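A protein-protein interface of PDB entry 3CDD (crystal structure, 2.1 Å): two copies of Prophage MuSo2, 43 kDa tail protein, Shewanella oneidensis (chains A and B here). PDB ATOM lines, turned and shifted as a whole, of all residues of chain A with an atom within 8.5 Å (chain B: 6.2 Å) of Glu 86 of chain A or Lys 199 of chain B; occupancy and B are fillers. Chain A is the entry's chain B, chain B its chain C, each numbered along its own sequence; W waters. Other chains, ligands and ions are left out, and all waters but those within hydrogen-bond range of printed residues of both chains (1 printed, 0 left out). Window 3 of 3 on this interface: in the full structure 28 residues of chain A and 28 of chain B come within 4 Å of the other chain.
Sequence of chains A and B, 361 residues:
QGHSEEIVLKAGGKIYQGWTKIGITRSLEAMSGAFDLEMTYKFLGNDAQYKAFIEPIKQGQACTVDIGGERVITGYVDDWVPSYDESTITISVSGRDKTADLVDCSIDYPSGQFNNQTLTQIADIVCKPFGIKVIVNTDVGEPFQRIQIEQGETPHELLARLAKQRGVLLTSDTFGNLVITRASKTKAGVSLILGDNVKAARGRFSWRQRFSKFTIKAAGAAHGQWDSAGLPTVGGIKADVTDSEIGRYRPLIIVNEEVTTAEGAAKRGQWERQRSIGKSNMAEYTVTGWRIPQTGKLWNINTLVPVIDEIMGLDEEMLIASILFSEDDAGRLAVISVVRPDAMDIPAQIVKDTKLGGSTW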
ATOM      1  N   TYR A  41      14.733  17.569  -0.859  1.00  0.00           N
ATOM      2  CA  TYR A  41      14.552  18.390   0.339  1.00  0.00           C
ATOM      3  C   TYR A  41      13.597  19.515  -0.032  1.00  0.00           C
ATOM      4  O   TYR A  41      13.803  20.195  -1.045  1.00  0.00           O
ATOM      5  CB  TYR A  41      15.879  18.995   0.786  1.00  0.00           C
ATOM      6  CG  TYR A  41      16.930  17.993   1.216  1.00  0.00           C
ATOM      7  CD1 TYR A  41      17.647  17.257   0.269  1.00  0.00           C
ATOM      8  CD2 TYR A  41      17.214  17.789   2.577  1.00  0.00           C
ATOM      9  CE1 TYR A  41      18.617  16.322   0.651  1.00  0.00           C
ATOM     10  CE2 TYR A  41      18.198  16.861   2.983  1.00  0.00           C
ATOM     11  CZ  TYR A  41      18.895  16.135   2.003  1.00  0.00           C
ATOM     12  OH  TYR A  41      19.870  15.228   2.372  1.00  0.00           O
ATOM     13  N   LYS A  42      12.560  19.689   0.786  1.00  0.00           N
ATOM     14  CA  LYS A  42      11.491  20.669   0.582  1.00  0.00           C
ATOM     15  C   LYS A  42      11.498  21.735   1.683  1.00  0.00           C
ATOM     16  O   LYS A  42      12.230  21.611   2.666  1.00  0.00           O
ATOM     17  CB  LYS A  42      10.130  19.976   0.610  1.00  0.00           C
ATOM     18  CG  LYS A  42       9.820  19.043  -0.538  1.00  0.00           C
ATOM     19  CD  LYS A  42       8.555  18.218  -0.240  1.00  0.00           C
ATOM     20  CE  LYS A  42       7.339  19.103   0.012  1.00  0.00           C
ATOM     21  NZ  LYS A  42       6.057  18.317   0.164  1.00  0.00           N
ATOM     22  N   PHE A  43      10.659  22.761   1.507  1.00  0.00           N
ATOM     23  CA  PHE A  43      10.501  23.914   2.435  1.00  0.00           C
ATOM     24  C   PHE A  43      11.823  24.558   2.816  1.00  0.00           C
ATOM     25  O   PHE A  43      12.049  24.880   3.974  1.00  0.00           O
ATOM     26  CB  PHE A  43       9.713  23.535   3.706  1.00  0.00           C
ATOM     27  CG  PHE A  43       8.550  22.629   3.451  1.00  0.00           C
ATOM     28  CD1 PHE A  43       7.436  23.079   2.753  1.00  0.00           C
ATOM     29  CD2 PHE A  43       8.574  21.313   3.897  1.00  0.00           C
ATOM     30  CE1 PHE A  43       6.366  22.213   2.495  1.00  0.00           C
ATOM     31  CE2 PHE A  43       7.496  20.454   3.653  1.00  0.00           C
ATOM     32  CZ  PHE A  43       6.400  20.911   2.952  1.00  0.00           C
ATOM     33  N   LEU A  44      12.698  24.749   1.836  1.00  0.00           N
ATOM     34  CA  LEU A  44      14.038  25.231   2.124  1.00  0.00           C
ATOM     35  C   LEU A  44      14.039  26.710   2.487  1.00  0.00           C
ATOM     36  O   LEU A  44      13.326  27.508   1.869  1.00  0.00           O
ATOM     37  CB  LEU A  44      14.980  24.959   0.944  1.00  0.00           C
ATOM     38  CG  LEU A  44      15.184  23.500   0.546  1.00  0.00           C
ATOM     39  CD1 LEU A  44      15.920  23.429  -0.775  1.00  0.00           C
ATOM     40  CD2 LEU A  44      15.903  22.716   1.653  1.00  0.00           C
ATOM     41  N   GLY A  45      14.840  27.055   3.499  1.00  0.00           N
ATOM     42  CA  GLY A  45      15.036  28.432   3.938  1.00  0.00           C
ATOM     43  C   GLY A  45      15.637  29.324   2.864  1.00  0.00           C
ATOM     44  O   GLY A  45      15.950  28.869   1.768  1.00  0.00           O
ATOM     45  N   ASN A  46      15.807  30.603   3.181  1.00  0.00           N
ATOM     46  CA  ASN A  46      16.239  31.577   2.187  1.00  0.00           C
ATOM     47  C   ASN A  46      17.698  31.373   1.788  1.00  0.00           C
ATOM     48  O   ASN A  46      18.075  31.552   0.611  1.00  0.00           O
ATOM     49  CB  ASN A  46      16.020  32.999   2.701  1.00  0.00           C
ATOM     50  CG  ASN A  46      15.519  33.948   1.612  1.00  0.00           C
ATOM     51  OD1 ASN A  46      15.663  33.682   0.409  1.00  0.00           O
ATOM     52  ND2 ASN A  46      14.923  35.062   2.037  1.00  0.00           N
ATOM     53  N   ASP A  47      18.515  30.985   2.763  1.00  0.00           N
ATOM     54  CA  ASP A  47      19.926  30.744   2.505  1.00  0.00           C
ATOM     55  C   ASP A  47      20.205  29.300   2.040  1.00  0.00           C
ATOM     56  O   ASP A  47      21.160  29.069   1.280  1.00  0.00           O
ATOM     57  CB  ASP A  47      20.812  31.253   3.671  1.00  0.00           C
ATOM     58  CG  ASP A  47      20.972  32.789   3.656  1.00  0.00           C
ATOM     59  OD1 ASP A  47      20.635  33.425   2.628  1.00  0.00           O
ATOM     60  OD2 ASP A  47      21.426  33.377   4.660  1.00  0.00           O
ATOM     61  N   ALA A  48      19.334  28.357   2.433  1.00  0.00           N
ATOM     62  CA  ALA A  48      19.416  26.953   1.975  1.00  0.00           C
ATOM     63  C   ALA A  48      19.023  26.687   0.502  1.00  0.00           C
ATOM     64  O   ALA A  48      19.497  25.720  -0.106  1.00  0.00           O
ATOM     65  CB  ALA A  48      18.626  26.052   2.890  1.00  0.00           C
ATOM     66  N   GLN A  49      18.156  27.533  -0.057  1.00  0.00           N
ATOM     67  CA  GLN A  49      17.688  27.384  -1.437  1.00  0.00           C
ATOM     68  C   GLN A  49      18.819  27.573  -2.465  1.00  0.00           C
ATOM     69  O   GLN A  49      19.778  28.296  -2.204  1.00  0.00           O
ATOM     70  CB  GLN A  49      16.522  28.338  -1.712  1.00  0.00           C
ATOM     71  CG  GLN A  49      16.907  29.830  -1.693  1.00  0.00           C
ATOM     72  CD  GLN A  49      15.783  30.755  -2.170  1.00  0.00           C
ATOM     73  OE1 GLN A  49      14.627  30.344  -2.284  1.00  0.00           O
ATOM     74  NE2 GLN A  49      16.131  32.010  -2.463  1.00  0.00           N
ATOM     75  N   TYR A  50      18.716  26.906  -3.621  1.00  0.00           N
ATOM     76  CA  TYR A  50      19.696  27.069  -4.711  1.00  0.00           C
ATOM     77  C   TYR A  50      21.133  26.719  -4.314  1.00  0.00           C
ATOM     78  O   TYR A  50      22.079  27.318  -4.810  1.00  0.00           O
ATOM     79  CB  TYR A  50      19.649  28.492  -5.299  1.00  0.00           C
ATOM     80  CG  TYR A  50      18.284  28.933  -5.760  1.00  0.00           C
ATOM     81  CD1 TYR A  50      17.711  30.103  -5.269  1.00  0.00           C
ATOM     82  CD2 TYR A  50      17.545  28.164  -6.673  1.00  0.00           C
ATOM     83  CE1 TYR A  50      16.441  30.497  -5.670  1.00  0.00           C
ATOM     84  CE2 TYR A  50      16.294  28.558  -7.085  1.00  0.00           C
ATOM     85  CZ  TYR A  50      15.741  29.727  -6.578  1.00  0.00           C
ATOM     86  OH  TYR A  50      14.485  30.122  -6.997  1.00  0.00           O
ATOM     87  N   SER A  83      17.075  18.704 -10.258  1.00  0.00           N
ATOM     88  CA  SER A  83      16.033  19.720 -10.400  1.00  0.00           C
ATOM     89  C   SER A  83      15.818  20.500  -9.110  1.00  0.00           C
ATOM     90  O   SER A  83      16.190  20.034  -8.017  1.00  0.00           O
ATOM     91  CB  SER A  83      14.721  19.099 -10.920  1.00  0.00           C
ATOM     92  OG  SER A  83      14.003  18.471  -9.880  1.00  0.00           O
ATOM     93  N   TYR A  84      15.263  21.709  -9.238  1.00  0.00           N
ATOM     94  CA  TYR A  84      15.088  22.604  -8.092  1.00  0.00           C
ATOM     95  C   TYR A  84      14.177  23.750  -8.437  1.00  0.00           C
ATOM     96  O   TYR A  84      13.925  24.034  -9.613  1.00  0.00           O
ATOM     97  CB  TYR A  84      16.429  23.167  -7.555  1.00  0.00           C
ATOM     98  CG  TYR A  84      17.259  23.880  -8.587  1.00  0.00           C
ATOM     99  CD1 TYR A  84      17.092  25.240  -8.829  1.00  0.00           C
ATOM    100  CD2 TYR A  84      18.222  23.187  -9.337  1.00  0.00           C
ATOM    101  CE1 TYR A  84      17.848  25.891  -9.795  1.00  0.00           C
ATOM    102  CE2 TYR A  84      18.991  23.837 -10.299  1.00  0.00           C
ATOM    103  CZ  TYR A  84      18.799  25.180 -10.528  1.00  0.00           C
ATOM    104  OH  TYR A  84      19.586  25.832 -11.485  1.00  0.00           O
ATOM    105  N   ASP A  85      13.676  24.391  -7.387  1.00  0.00           N
ATOM    106  CA  ASP A  85      12.899  25.600  -7.506  1.00  0.00           C
ATOM    107  C   ASP A  85      13.168  26.462  -6.291  1.00  0.00           C
ATOM    108  O   ASP A  85      14.207  26.300  -5.637  1.00  0.00           O
ATOM    109  CB  ASP A  85      11.409  25.301  -7.752  1.00  0.00           C
ATOM    110  CG  ASP A  85      10.741  24.506  -6.625  1.00  0.00           C
ATOM    111  OD1 ASP A  85      11.085  24.685  -5.431  1.00  0.00           O
ATOM    112  OD2 ASP A  85       9.832  23.710  -6.950  1.00  0.00           O
ATOM    113  N   GLU A  86      12.257  27.385  -6.000  1.00  0.00           N
ATOM    114  CA  GLU A  86      12.434  28.340  -4.904  1.00  0.00           C
ATOM    115  C   GLU A  86      12.478  27.700  -3.505  1.00  0.00           C
ATOM    116  O   GLU A  86      13.151  28.220  -2.622  1.00  0.00           O
ATOM    117  CB  GLU A  86      11.345  29.428  -4.953  1.00  0.00           C
ATOM    118  CG  GLU A  86      11.653  30.531  -5.974  1.00  0.00           C
ATOM    119  CD  GLU A  86      10.421  31.296  -6.461  1.00  0.00           C
ATOM    120  OE1 GLU A  86       9.578  30.701  -7.184  1.00  0.00           O
ATOM    121  OE2 GLU A  86      10.316  32.501  -6.146  1.00  0.00           O
ATOM    122  N   SER A  87      11.766  26.587  -3.298  1.00  0.00           N
ATOM    123  CA  SER A  87      11.741  25.981  -1.972  1.00  0.00           C
ATOM    124  C   SER A  87      12.170  24.504  -1.919  1.00  0.00           C
ATOM    125  O   SER A  87      12.055  23.859  -0.857  1.00  0.00           O
ATOM    126  CB  SER A  87      10.373  26.192  -1.319  1.00  0.00           C
ATOM    127  OG  SER A  87       9.345  25.629  -2.114  1.00  0.00           O
ATOM    128  N   THR A  88      12.679  23.992  -3.048  1.00  0.00           N
ATOM    129  CA  THR A  88      12.983  22.568  -3.225  1.00  0.00           C
ATOM    130  C   THR A  88      14.265  22.336  -4.017  1.00  0.00           C
ATOM    131  O   THR A  88      14.605  23.128  -4.900  1.00  0.00           O
ATOM    132  CB  THR A  88      11.856  21.852  -4.028  1.00  0.00           C
ATOM    133  OG1 THR A  88      10.596  22.292  -3.541  1.00  0.00           O
ATOM    134  CG2 THR A  88      11.922  20.344  -3.853  1.00  0.00           C
ATOM    135  N   ILE A  89      14.966  21.247  -3.686  1.00  0.00           N
ATOM    136  CA  ILE A  89      16.043  20.672  -4.521  1.00  0.00           C
ATOM    137  C   ILE A  89      15.838  19.152  -4.587  1.00  0.00           C
ATOM    138  O   ILE A  89      15.671  18.495  -3.541  1.00  0.00           O
ATOM    139  CB  ILE A  89      17.489  21.017  -3.991  1.00  0.00           C
ATOM    140  CG1 ILE A  89      17.709  22.531  -3.929  1.00  0.00           C
ATOM    141  CG2 ILE A  89      18.571  20.385  -4.883  1.00  0.00           C
ATOM    142  CD1 ILE A  89      18.754  22.982  -2.883  1.00  0.00           C
ATOM    143  N   ASN B 197      19.472  34.588 -11.111  1.00  0.00           N
ATOM    144  CA  ASN B 197      18.316  34.884 -11.971  1.00  0.00           C
ATOM    145  C   ASN B 197      17.459  33.654 -12.355  1.00  0.00           C
ATOM    146  O   ASN B 197      16.471  33.781 -13.077  1.00  0.00           O
ATOM    147  CB  ASN B 197      18.762  35.674 -13.216  1.00  0.00           C
ATOM    148  CG  ASN B 197      19.729  34.890 -14.103  1.00  0.00           C
ATOM    149  OD1 ASN B 197      20.421  33.982 -13.636  1.00  0.00           O
ATOM    150  ND2 ASN B 197      19.778  35.244 -15.396  1.00  0.00           N
ATOM    151  N   VAL B 198      17.840  32.479 -11.849  1.00  0.00           N
ATOM    152  CA  VAL B 198      17.140  31.217 -12.114  1.00  0.00           C
ATOM    153  C   VAL B 198      16.060  30.989 -11.058  1.00  0.00           C
ATOM    154  O   VAL B 198      16.360  30.839  -9.872  1.00  0.00           O
ATOM    155  CB  VAL B 198      18.147  30.012 -12.153  1.00  0.00           C
ATOM    156  CG1 VAL B 198      17.430  28.662 -12.304  1.00  0.00           C
ATOM    157  CG2 VAL B 198      19.165  30.203 -13.304  1.00  0.00           C
ATOM    158  N   LYS B 199      14.802  30.973 -11.496  1.00  0.00           N
ATOM    159  CA  LYS B 199      13.674  30.686 -10.614  1.00  0.00           C
ATOM    160  C   LYS B 199      13.599  29.185 -10.293  1.00  0.00           C
ATOM    161  O   LYS B 199      13.522  28.780  -9.131  1.00  0.00           O
ATOM    162  CB  LYS B 199      12.370  31.160 -11.277  1.00  0.00           C
ATOM    163  CG  LYS B 199      11.154  31.213 -10.366  1.00  0.00           C
ATOM    164  CD  LYS B 199       9.875  31.232 -11.218  1.00  0.00           C
ATOM    165  CE  LYS B 199       8.624  30.910 -10.403  1.00  0.00           C
ATOM    166  NZ  LYS B 199       7.950  32.124  -9.863  1.00  0.00           N
ATOM    167  N   ALA B 200      13.596  28.383 -11.348  1.00  0.00           N
ATOM    168  CA  ALA B 200      13.613  26.921 -11.272  1.00  0.00           C
ATOM    169  C   ALA B 200      14.403  26.373 -12.460  1.00  0.00           C
ATOM    170  O   ALA B 200      14.545  27.043 -13.490  1.00  0.00           O
ATOM    171  CB  ALA B 200      12.193  26.359 -11.269  1.00  0.00           C
ATOM    172  N   ALA B 201      14.931  25.162 -12.313  1.00  0.00           N
ATOM    173  CA  ALA B 201      15.617  24.479 -13.413  1.00  0.00           C
ATOM    174  C   ALA B 201      15.414  22.984 -13.276  1.00  0.00           C
ATOM    175  O   ALA B 201      15.053  22.504 -12.204  1.00  0.00           O
ATOM    176  CB  ALA B 201      17.101  24.809 -13.423  1.00  0.00           C
ATOM    177  N   THR B 286      14.075  28.110 -15.891  1.00  0.00           N
ATOM    178  CA  THR B 286      12.906  28.984 -15.757  1.00  0.00           C
ATOM    179  C   THR B 286      13.371  30.305 -15.165  1.00  0.00           C
ATOM    180  O   THR B 286      14.027  30.336 -14.122  1.00  0.00           O
ATOM    181  CB  THR B 286      11.769  28.310 -14.919  1.00  0.00           C
ATOM    182  OG1 THR B 286      11.435  27.049 -15.518  1.00  0.00           O
ATOM    183  CG2 THR B 286      10.498  29.162 -14.887  1.00  0.00           C
ATOM    184  N   VAL B 287      13.045  31.389 -15.873  1.00  0.00           N
ATOM    185  CA  VAL B 287      13.308  32.757 -15.442  1.00  0.00           C
ATOM    186  C   VAL B 287      11.996  33.539 -15.471  1.00  0.00           C
ATOM    187  O   VAL B 287      11.053  33.166 -16.165  1.00  0.00           O
ATOM    188  CB  VAL B 287      14.377  33.496 -16.345  1.00  0.00           C
ATOM    189  CG1 VAL B 287      15.762  32.820 -16.251  1.00  0.00           C
ATOM    190  CG2 VAL B 287      13.914  33.583 -17.789  1.00  0.00           C
ATOM    191  N   THR B 288      11.959  34.623 -14.706  1.00  0.00           N
ATOM    192  CA  THR B 288      10.819  35.541 -14.630  1.00  0.00           C
ATOM    193  C   THR B 288      10.925  36.503 -15.814  1.00  0.00           C
ATOM    194  O   THR B 288      11.982  37.088 -16.030  1.00  0.00           O
ATOM    195  CB  THR B 288      10.861  36.311 -13.269  1.00  0.00           C
ATOM    196  OG1 THR B 288      10.717  35.374 -12.199  1.00  0.00           O
ATOM    197  CG2 THR B 288       9.750  37.376 -13.141  1.00  0.00           C
ATOM    198  N   LEU B 333       6.708  33.786 -17.477  1.00  0.00           N
ATOM    199  CA  LEU B 333       7.942  33.012 -17.347  1.00  0.00           C
ATOM    200  C   LEU B 333       8.527  32.731 -18.721  1.00  0.00           C
ATOM    201  O   LEU B 333       7.812  32.727 -19.697  1.00  0.00           O
ATOM    202  CB  LEU B 333       7.666  31.680 -16.637  1.00  0.00           C
ATOM    203  CG  LEU B 333       7.027  31.678 -15.250  1.00  0.00           C
ATOM    204  CD1 LEU B 333       6.658  30.258 -14.897  1.00  0.00           C
ATOM    205  CD2 LEU B 333       7.950  32.262 -14.196  1.00  0.00           C
HETATM  206  O   HOH W   1      12.028  22.305 -11.101  1.00  0.00           O
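Water W1 lies within hydrogen-bond range of the backbone carbonyl oxygen (O) of Tyr 84 of chain A (3.0 Å) and the backbone carbonyl oxygen (O) of Ala 201 of chain B (3.2 Å).
O of Glu 86 of chain A lies close to OE1 of Gln 49 of chain A, 2.6 Å away.
OD1 of Asp 85 of chain A sits at hydrogen-bond distance from N of Ser 87 of chain A.
The side-chain carboxylate (OD1) of Asp 85 of chain A is in hydrogen-bond range of the backbone NH (N) of Thr 88 of chain A, 2.9 Å away.
The backbone NH (N) of Lys 199 of chain B sits at hydrogen-bond distance from the backbone carbonyl oxygen (O) of Thr 286 of chain B (2.8 Å).
O of Ala 200 of chain B is in hydrogen-bond range of N of Thr 286 of chain B (2.7 Å).
Asp 47 of chain A touches none of the printed residues of chain B.
Of the printed residues of chain B, Asp 85 of chain A touches Lys 199 and Ala 200.
Glu 86 of chain A touches just one residue of chain B: Lys 199.
Of the printed residues of chain A, Val 198 of chain B touches Tyr 50 (3.5 Å) and Tyr 84 (3.7 Å).
Of chain A, only Tyr 50 (2.7 Å), Asp 85 (3.6 Å) and Glu 86 (3.4 Å) come within 4 Å of Lys 199 of chain B.
Printed residues of chain A within 4 Å of Ala 200 of chain B: Tyr 84 (3.3 Å) and Asp 85 (3.8 Å).
Of the printed residues of chain A, Ala 201 of chain B touches Ser 83 (3.5 Å) and Tyr 84 (3.1 Å).
Hydrophobic or aromatic side chains of chain B within 4 Å of the printed part of chain A: Val 198, Ala 200 and Ala 201.
OH of Tyr 50 of chain A is in hydrogen-bond range of O of Lys 199 of chain B, at 2.7 Å.
The backbone carbonyl oxygen (O) of Ala 201 of chain B is in hydrogen-bond range of the backbone NH (N) of Tyr 84 of chain A (3.1 Å).
OE1 of Glu 86 of chain A lies within salt-bridge range of NZ of Lys 199 of chain B.
OH of Tyr 50 of chain A touches O of Val 198 of chain B (3.5 Å).
CA of Ser 83 of chain A touches O of Ala 201 of chain B, at 3.5 Å.
Val 198 of chain B touches Tyr 84 of chain A.
O of Tyr 84 of chain A touches CB of Ala 200 of chain B, 3.3 Å away.
Asp 85 of chain A touches Lys 199 of chain B.
CB of Asp 85 of chain A touches CB of Ala 200 of chain B, 3.8 Å away.
No position is printed for both chains.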
